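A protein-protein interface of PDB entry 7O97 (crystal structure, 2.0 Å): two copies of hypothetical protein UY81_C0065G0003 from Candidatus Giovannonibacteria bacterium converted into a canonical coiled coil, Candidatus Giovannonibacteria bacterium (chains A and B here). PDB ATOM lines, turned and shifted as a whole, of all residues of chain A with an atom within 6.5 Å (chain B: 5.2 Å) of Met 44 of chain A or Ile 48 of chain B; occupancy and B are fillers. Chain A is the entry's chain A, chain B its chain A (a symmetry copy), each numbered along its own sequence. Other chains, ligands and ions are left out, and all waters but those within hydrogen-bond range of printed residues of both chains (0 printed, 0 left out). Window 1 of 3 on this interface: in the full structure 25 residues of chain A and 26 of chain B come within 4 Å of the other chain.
Ile 41 of chain B touches Met 44 of chain A (CG2 to CE, 3.5 Å).
Met 44 of chain A touches Met 44 of chain B (SD to CB, 3.7 Å).
Met 44 of chain A touches Ile 48 of chain B.
Ile 48 of chain B touches Asp 47 of chain A.
Ile 48 of chain A touches Ile 48 of chain B (CG1 to CD1, 3.5 Å).
Ile 48 of chain B touches Leu 51 of chain A (CG2 to CD1, 3.9 Å).
CD2 of Leu 51 of chain A touches CA of Asp 52 of chain B, at 3.95 Å.
Met 44 of chain A touches Ile 41 of chain B, but with the chains exchanged Ile 41 of chain A does not touch Met 44 of chain B (7.1 Å).
Met 44 of chain B touches its own counterpart, Met 44 of chain A.
Ile 48 of chain A touches its own counterpart, Ile 48 of chain B.
Leu 51 of chain A touches Ile 48 of chain B, but with the chains exchanged Ile 48 of chain A does not touch Leu 51 of chain B (6.4 Å).
Of the 8 pairs that touch across the chains among the printed residues, 2 have their exchanged pair printed and touching as well.
Of the printed residues of chain B, Asp 47 of chain A touches Ile 48 (3.8 Å).
Of the printed residues of chain A, Ile 41 of chain B touches Met 44.
Of the printed residues of chain A, Lys 45 of chain B touches Met 44.
Of chain A, only Met 44 (3.2 Å), Asp 47 (3.8 Å), Ile 48 (3.5 Å) and Leu 51 (3.9 Å) come within 4 Å of Ile 48 of chain B.
Printed residues of chain A within 4 Å of Asp 52 of chain B: Leu 51.
The nearest residue of chain A that does not touch Ile 48 of chain B is Lys 45 of chain A (5.8 Å).
Hydrophobic or aromatic side chains of chain B within 4 Å of the printed part of chain A: Ile 41, Met 44 and Ile 48.
Printed residues of chain A that touch a printed residue of chain B: Met 44, Asp 47, Ile 48 and Leu 51.
Hydrophobic or aromatic side chains of chain A within 4 Å of the printed part of chain B: Met 44, Ile 48 and Leu 51.
The backbone NH of Lys 45 of chain B lies close to the side-chain sulfur of Met 44 of chain A.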
ATOM      1  N   LYS A  39     -12.061 -29.027 -21.642  1.00  0.00           N
ATOM      2  CA  LYS A  39     -13.049 -28.201 -22.233  1.00  0.00           C
ATOM      3  C   LYS A  39     -13.530 -27.179 -21.190  1.00  0.00           C
ATOM      4  O   LYS A  39     -13.622 -26.013 -21.523  1.00  0.00           O
ATOM      5  CB  LYS A  39     -14.194 -29.054 -22.798  1.00  0.00           C
ATOM      6  CG  LYS A  39     -14.936 -28.477 -24.005  1.00  0.00           C
ATOM      7  CD  LYS A  39     -16.228 -29.257 -24.375  1.00  0.00           C
ATOM      8  CE  LYS A  39     -16.247 -30.754 -24.033  1.00  0.00           C
ATOM      9  NZ  LYS A  39     -15.330 -31.616 -24.835  1.00  0.00           N
ATOM     10  N   ASP A  40     -13.799 -27.580 -19.934  1.00  0.00           N
ATOM     11  CA  ASP A  40     -14.212 -26.580 -18.874  1.00  0.00           C
ATOM     12  C   ASP A  40     -13.211 -25.445 -18.720  1.00  0.00           C
ATOM     13  O   ASP A  40     -13.584 -24.268 -18.573  1.00  0.00           O
ATOM     14  CB  ASP A  40     -14.402 -27.256 -17.509  1.00  0.00           C
ATOM     15  CG  ASP A  40     -15.705 -28.026 -17.417  1.00  0.00           C
ATOM     16  OD1 ASP A  40     -16.493 -28.108 -18.408  1.00  0.00           O
ATOM     17  OD2 ASP A  40     -15.932 -28.560 -16.338  1.00  0.00           O
ATOM     18  N   ILE A  41     -11.945 -25.811 -18.743  1.00  0.00           N
ATOM     19  CA  ILE A  41     -10.879 -24.842 -18.640  1.00  0.00           C
ATOM     20  C   ILE A  41     -10.822 -23.878 -19.822  1.00  0.00           C
ATOM     21  O   ILE A  41     -10.592 -22.695 -19.628  1.00  0.00           O
ATOM     22  CB  ILE A  41      -9.530 -25.569 -18.464  1.00  0.00           C
ATOM     23  CG1 ILE A  41      -9.429 -26.085 -17.050  1.00  0.00           C
ATOM     24  CG2 ILE A  41      -8.353 -24.630 -18.697  1.00  0.00           C
ATOM     25  CD1 ILE A  41      -8.316 -27.090 -16.920  1.00  0.00           C
ATOM     26  N   ALA A  42     -11.012 -24.376 -21.055  1.00  0.00           N
ATOM     27  CA  ALA A  42     -11.066 -23.492 -22.245  1.00  0.00           C
ATOM     28  C   ALA A  42     -12.163 -22.445 -22.068  1.00  0.00           C
ATOM     29  O   ALA A  42     -11.980 -21.273 -22.354  1.00  0.00           O
ATOM     30  CB  ALA A  42     -11.284 -24.319 -23.531  1.00  0.00           C
ATOM     31  N   GLY A  43     -13.296 -22.886 -21.514  1.00  0.00           N
ATOM     32  CA  GLY A  43     -14.405 -22.017 -21.239  1.00  0.00           C
ATOM     33  C   GLY A  43     -14.091 -21.001 -20.150  1.00  0.00           C
ATOM     34  O   GLY A  43     -14.626 -19.876 -20.169  1.00  0.00           O
ATOM     35  N   MET A  44     -13.282 -21.397 -19.168  1.00  0.00           N
ATOM     36  CA  MET A  44     -13.029 -20.549 -17.998  1.00  0.00           C
ATOM     37  C   MET A  44     -12.012 -19.476 -18.404  1.00  0.00           C
ATOM     38  O   MET A  44     -12.139 -18.285 -18.080  1.00  0.00           O
ATOM     39  CB  MET A  44     -12.527 -21.490 -16.853  1.00  0.00           C
ATOM     40  CG  MET A  44     -12.933 -21.078 -15.427  1.00  0.00           C
ATOM     41  SD  MET A  44     -13.119 -22.455 -14.244  1.00  0.00           S
ATOM     42  CE  MET A  44     -14.071 -23.570 -15.286  1.00  0.00           C
ATOM     43  N   LYS A  45     -10.994 -19.886 -19.136  1.00  0.00           N
ATOM     44  CA  LYS A  45     -10.060 -18.921 -19.714  1.00  0.00           C
ATOM     45  C   LYS A  45     -10.765 -17.854 -20.555  1.00  0.00           C
ATOM     46  O   LYS A  45     -10.300 -16.691 -20.613  1.00  0.00           O
ATOM     47  CB  LYS A  45      -9.019 -19.635 -20.559  1.00  0.00           C
ATOM     48  CG  LYS A  45      -7.917 -20.262 -19.727  1.00  0.00           C
ATOM     49  CD  LYS A  45      -6.667 -20.595 -20.558  1.00  0.00           C
ATOM     50  CE  LYS A  45      -5.608 -21.410 -19.817  1.00  0.00           C
ATOM     51  NZ  LYS A  45      -4.257 -21.175 -20.409  1.00  0.00           N
ATOM     52  N   HIS A  46     -11.849 -18.238 -21.226  1.00  0.00           N
ATOM     53  CA  HIS A  46     -12.636 -17.309 -22.038  1.00  0.00           C
ATOM     54  C   HIS A  46     -13.406 -16.386 -21.153  1.00  0.00           C
ATOM     55  O   HIS A  46     -13.441 -15.216 -21.438  1.00  0.00           O
ATOM     56  CB  HIS A  46     -13.652 -18.049 -22.923  1.00  0.00           C
ATOM     57  CG  HIS A  46     -14.684 -17.156 -23.565  1.00  0.00           C
ATOM     58  ND1 HIS A  46     -14.373 -16.183 -24.497  1.00  0.00           N
ATOM     59  CD2 HIS A  46     -16.031 -17.096 -23.393  1.00  0.00           C
ATOM     60  CE1 HIS A  46     -15.483 -15.567 -24.871  1.00  0.00           C
ATOM     61  NE2 HIS A  46     -16.502 -16.105 -24.220  1.00  0.00           N
ATOM     62  N   ASP A  47     -14.068 -16.917 -20.111  1.00  0.00           N
ATOM     63  CA  ASP A  47     -14.795 -16.075 -19.138  1.00  0.00           C
ATOM     64  C   ASP A  47     -13.842 -15.059 -18.462  1.00  0.00           C
ATOM     65  O   ASP A  47     -14.211 -13.933 -18.261  1.00  0.00           O
ATOM     66  CB  ASP A  47     -15.537 -16.892 -18.027  1.00  0.00           C
ATOM     67  CG  ASP A  47     -16.617 -17.899 -18.553  1.00  0.00           C
ATOM     68  OD1 ASP A  47     -17.473 -17.550 -19.410  1.00  0.00           O
ATOM     69  OD2 ASP A  47     -16.639 -19.039 -18.032  1.00  0.00           O
ATOM     70  N   ILE A  48     -12.620 -15.461 -18.122  1.00  0.00           N
ATOM     71  CA  ILE A  48     -11.644 -14.558 -17.495  1.00  0.00           C
ATOM     72  C   ILE A  48     -11.263 -13.413 -18.485  1.00  0.00           C
ATOM     73  O   ILE A  48     -11.319 -12.208 -18.144  1.00  0.00           O
ATOM     74  CB  ILE A  48     -10.432 -15.368 -16.980  1.00  0.00           C
ATOM     75  CG1 ILE A  48     -10.904 -16.234 -15.809  1.00  0.00           C
ATOM     76  CG2 ILE A  48      -9.267 -14.456 -16.635  1.00  0.00           C
ATOM     77  CD1 ILE A  48      -9.884 -17.186 -15.239  1.00  0.00           C
ATOM     78  N   ALA A  49     -10.980 -13.784 -19.733  1.00  0.00           N
ATOM     79  CA  ALA A  49     -10.664 -12.840 -20.806  1.00  0.00           C
ATOM     80  C   ALA A  49     -11.785 -11.836 -21.072  1.00  0.00           C
ATOM     81  O   ALA A  49     -11.524 -10.683 -21.359  1.00  0.00           O
ATOM     82  CB  ALA A  49     -10.371 -13.604 -22.092  1.00  0.00           C
ATOM     83  N   LEU A  51     -14.082 -10.959 -18.698  1.00  0.00           N
ATOM     84  CA  LEU A  51     -14.070 -10.116 -17.507  1.00  0.00           C
ATOM     85  C   LEU A  51     -12.976  -9.081 -17.655  1.00  0.00           C
ATOM     86  O   LEU A  51     -13.225  -7.951 -17.343  1.00  0.00           O
ATOM     87  CB  LEU A  51     -13.835 -10.882 -16.214  1.00  0.00           C
ATOM     88  CG  LEU A  51     -14.954 -11.763 -15.679  1.00  0.00           C
ATOM     89  CD1 LEU A  51     -14.436 -12.704 -14.589  1.00  0.00           C
ATOM     90  CD2 LEU A  51     -16.110 -10.909 -15.164  1.00  0.00           C
ATOM     91  N   ILE B  41     -11.805 -26.560 -10.058  1.00  0.00           N
ATOM     92  CA  ILE B  41     -12.570 -25.929 -11.108  1.00  0.00           C
ATOM     93  C   ILE B  41     -13.949 -25.460 -10.653  1.00  0.00           C
ATOM     94  O   ILE B  41     -14.381 -24.385 -11.037  1.00  0.00           O
ATOM     95  CB  ILE B  41     -12.691 -26.887 -12.312  1.00  0.00           C
ATOM     96  CG1 ILE B  41     -11.375 -26.916 -13.052  1.00  0.00           C
ATOM     97  CG2 ILE B  41     -13.760 -26.424 -13.293  1.00  0.00           C
ATOM     98  CD1 ILE B  41     -11.318 -28.078 -14.006  1.00  0.00           C
ATOM     99  N   MET B  44     -13.423 -22.346  -9.022  1.00  0.00           N
ATOM    100  CA  MET B  44     -12.936 -21.259  -9.878  1.00  0.00           C
ATOM    101  C   MET B  44     -14.134 -20.688 -10.644  1.00  0.00           C
ATOM    102  O   MET B  44     -14.314 -19.468 -10.783  1.00  0.00           O
ATOM    103  CB  MET B  44     -11.829 -21.867 -10.803  1.00  0.00           C
ATOM    104  CG  MET B  44     -10.679 -20.917 -11.177  1.00  0.00           C
ATOM    105  SD  MET B  44      -9.073 -21.726 -11.488  1.00  0.00           S
ATOM    106  CE  MET B  44      -9.055 -22.829 -10.068  1.00  0.00           C
ATOM    107  N   LYS B  45     -14.981 -21.570 -11.141  1.00  0.00           N
ATOM    108  CA  LYS B  45     -16.240 -21.132 -11.744  1.00  0.00           C
ATOM    109  C   LYS B  45     -17.067 -20.255 -10.801  1.00  0.00           C
ATOM    110  O   LYS B  45     -17.791 -19.343 -11.263  1.00  0.00           O
ATOM    111  CB  LYS B  45     -17.060 -22.333 -12.181  1.00  0.00           C
ATOM    112  CG  LYS B  45     -16.588 -22.918 -13.497  1.00  0.00           C
ATOM    113  CD  LYS B  45     -17.644 -23.823 -14.153  1.00  0.00           C
ATOM    114  CE  LYS B  45     -17.149 -24.598 -15.375  1.00  0.00           C
ATOM    115  NZ  LYS B  45     -18.290 -24.936 -16.277  1.00  0.00           N
ATOM    116  N   HIS B  46     -16.997 -20.538  -9.501  1.00  0.00           N
ATOM    117  CA  HIS B  46     -17.709 -19.756  -8.491  1.00  0.00           C
ATOM    118  C   HIS B  46     -17.056 -18.424  -8.323  1.00  0.00           C
ATOM    119  O   HIS B  46     -17.757 -17.448  -8.242  1.00  0.00           O
ATOM    120  CB  HIS B  46     -17.693 -20.450  -7.119  1.00  0.00           C
ATOM    121  CG  HIS B  46     -18.151 -19.580  -5.976  1.00  0.00           C
ATOM    122  ND1 HIS B  46     -19.439 -19.087  -5.865  1.00  0.00           N
ATOM    123  CD2 HIS B  46     -17.474 -19.113  -4.893  1.00  0.00           C
ATOM    124  CE1 HIS B  46     -19.532 -18.358  -4.764  1.00  0.00           C
ATOM    125  NE2 HIS B  46     -18.357 -18.362  -4.155  1.00  0.00           N
ATOM    126  N   ASP B  47     -15.717 -18.388  -8.217  1.00  0.00           N
ATOM    127  CA  ASP B  47     -14.977 -17.113  -8.124  1.00  0.00           C
ATOM    128  C   ASP B  47     -15.250 -16.220  -9.359  1.00  0.00           C
ATOM    129  O   ASP B  47     -15.402 -15.036  -9.223  1.00  0.00           O
ATOM    130  CB  ASP B  47     -13.430 -17.291  -7.959  1.00  0.00           C
ATOM    131  CG  ASP B  47     -12.985 -18.092  -6.688  1.00  0.00           C
ATOM    132  OD1 ASP B  47     -13.464 -17.832  -5.552  1.00  0.00           O
ATOM    133  OD2 ASP B  47     -12.080 -18.948  -6.837  1.00  0.00           O
ATOM    134  N   ILE B  48     -15.320 -16.796 -10.557  1.00  0.00           N
ATOM    135  CA  ILE B  48     -15.596 -16.028 -11.780  1.00  0.00           C
ATOM    136  C   ILE B  48     -17.031 -15.417 -11.715  1.00  0.00           C
ATOM    137  O   ILE B  48     -17.233 -14.197 -11.924  1.00  0.00           O
ATOM    138  CB  ILE B  48     -15.350 -16.913 -13.025  1.00  0.00           C
ATOM    139  CG1 ILE B  48     -13.847 -17.187 -13.121  1.00  0.00           C
ATOM    140  CG2 ILE B  48     -15.937 -16.280 -14.274  1.00  0.00           C
ATOM    141  CD1 ILE B  48     -13.418 -18.132 -14.214  1.00  0.00           C
ATOM    142  N   ALA B  49     -18.003 -16.238 -11.322  1.00  0.00           N
ATOM    143  CA  ALA B  49     -19.394 -15.820 -11.145  1.00  0.00           C
ATOM    144  C   ALA B  49     -19.558 -14.701 -10.116  1.00  0.00           C
ATOM    145  O   ALA B  49     -20.378 -13.819 -10.290  1.00  0.00           O
ATOM    146  CB  ALA B  49     -20.239 -17.013 -10.714  1.00  0.00           C
ATOM    147  N   GLN B  50     -18.792 -14.762  -9.036  1.00  0.00           N
ATOM    148  CA  GLN B  50     -18.735 -13.681  -8.020  1.00  0.00           C
ATOM    149  C   GLN B  50     -18.102 -12.388  -8.542  1.00  0.00           C
ATOM    150  O   GLN B  50     -18.545 -11.294  -8.187  1.00  0.00           O
ATOM    151  CB  GLN B  50     -17.949 -14.140  -6.773  1.00  0.00           C
ATOM    152  CG  GLN B  50     -18.745 -14.828  -5.638  1.00  0.00           C
ATOM    153  CD  GLN B  50     -20.151 -14.273  -5.431  1.00  0.00           C
ATOM    154  OE1 GLN B  50     -21.146 -14.936  -5.747  1.00  0.00           O
ATOM    155  NE2 GLN B  50     -20.239 -13.058  -4.898  1.00  0.00           N
ATOM    156  N   LEU B  51     -17.044 -12.518  -9.345  1.00  0.00           N
ATOM    157  CA  LEU B  51     -16.436 -11.364 -10.002  1.00  0.00           C
ATOM    158  C   LEU B  51     -17.443 -10.764 -10.959  1.00  0.00           C
ATOM    159  O   LEU B  51     -17.557  -9.571 -10.980  1.00  0.00           O
ATOM    160  CB  LEU B  51     -15.172 -11.695 -10.779  1.00  0.00           C
ATOM    161  CG  LEU B  51     -13.906 -12.022 -10.002  1.00  0.00           C
ATOM    162  CD1 LEU B  51     -12.851 -12.653 -10.914  1.00  0.00           C
ATOM    163  CD2 LEU B  51     -13.362 -10.774  -9.313  1.00  0.00           C
ATOM    164  N   ASP B  52     -18.097 -11.582 -11.794  1.00  0.00           N
ATOM    165  CA  ASP B  52     -19.167 -11.109 -12.665  1.00  0.00           C
ATOM    166  C   ASP B  52     -20.181 -10.257 -11.846  1.00  0.00           C
ATOM    167  O   ASP B  52     -20.513  -9.163 -12.253  1.00  0.00           O
ATOM    168  CB  ASP B  52     -19.811 -12.306 -13.391  1.00  0.00           C
ATOM    169  CG  ASP B  52     -21.060 -11.933 -14.193  1.00  0.00           C
ATOM    170  OD1 ASP B  52     -20.946 -11.076 -15.088  1.00  0.00           O
ATOM    171  OD2 ASP B  52     -22.159 -12.491 -13.941  1.00  0.00           O
ATOM    172  N   LYS B  53     -20.601 -10.765 -10.684  1.00  0.00           N
ATOM    173  CA  LYS B  53     -21.508 -10.075  -9.750  1.00  0.00           C
ATOM    174  C   LYS B  53     -20.947  -8.700  -9.312  1.00  0.00           C
ATOM    175  O   LYS B  53     -21.631  -7.690  -9.398  1.00  0.00           O
ATOM    176  CB  LYS B  53     -21.741 -10.976  -8.515  1.00  0.00           C
ATOM    177  CG  LYS B  53     -23.199 -11.208  -8.055  1.00  0.00           C
ATOM    178  CD  LYS B  53     -23.421 -12.616  -7.430  1.00  0.00           C
ATOM    179  CE  LYS B  53     -22.839 -13.784  -8.271  1.00  0.00           C
ATOM    180  NZ  LYS B  53     -23.163 -15.231  -7.972  1.00  0.00           N
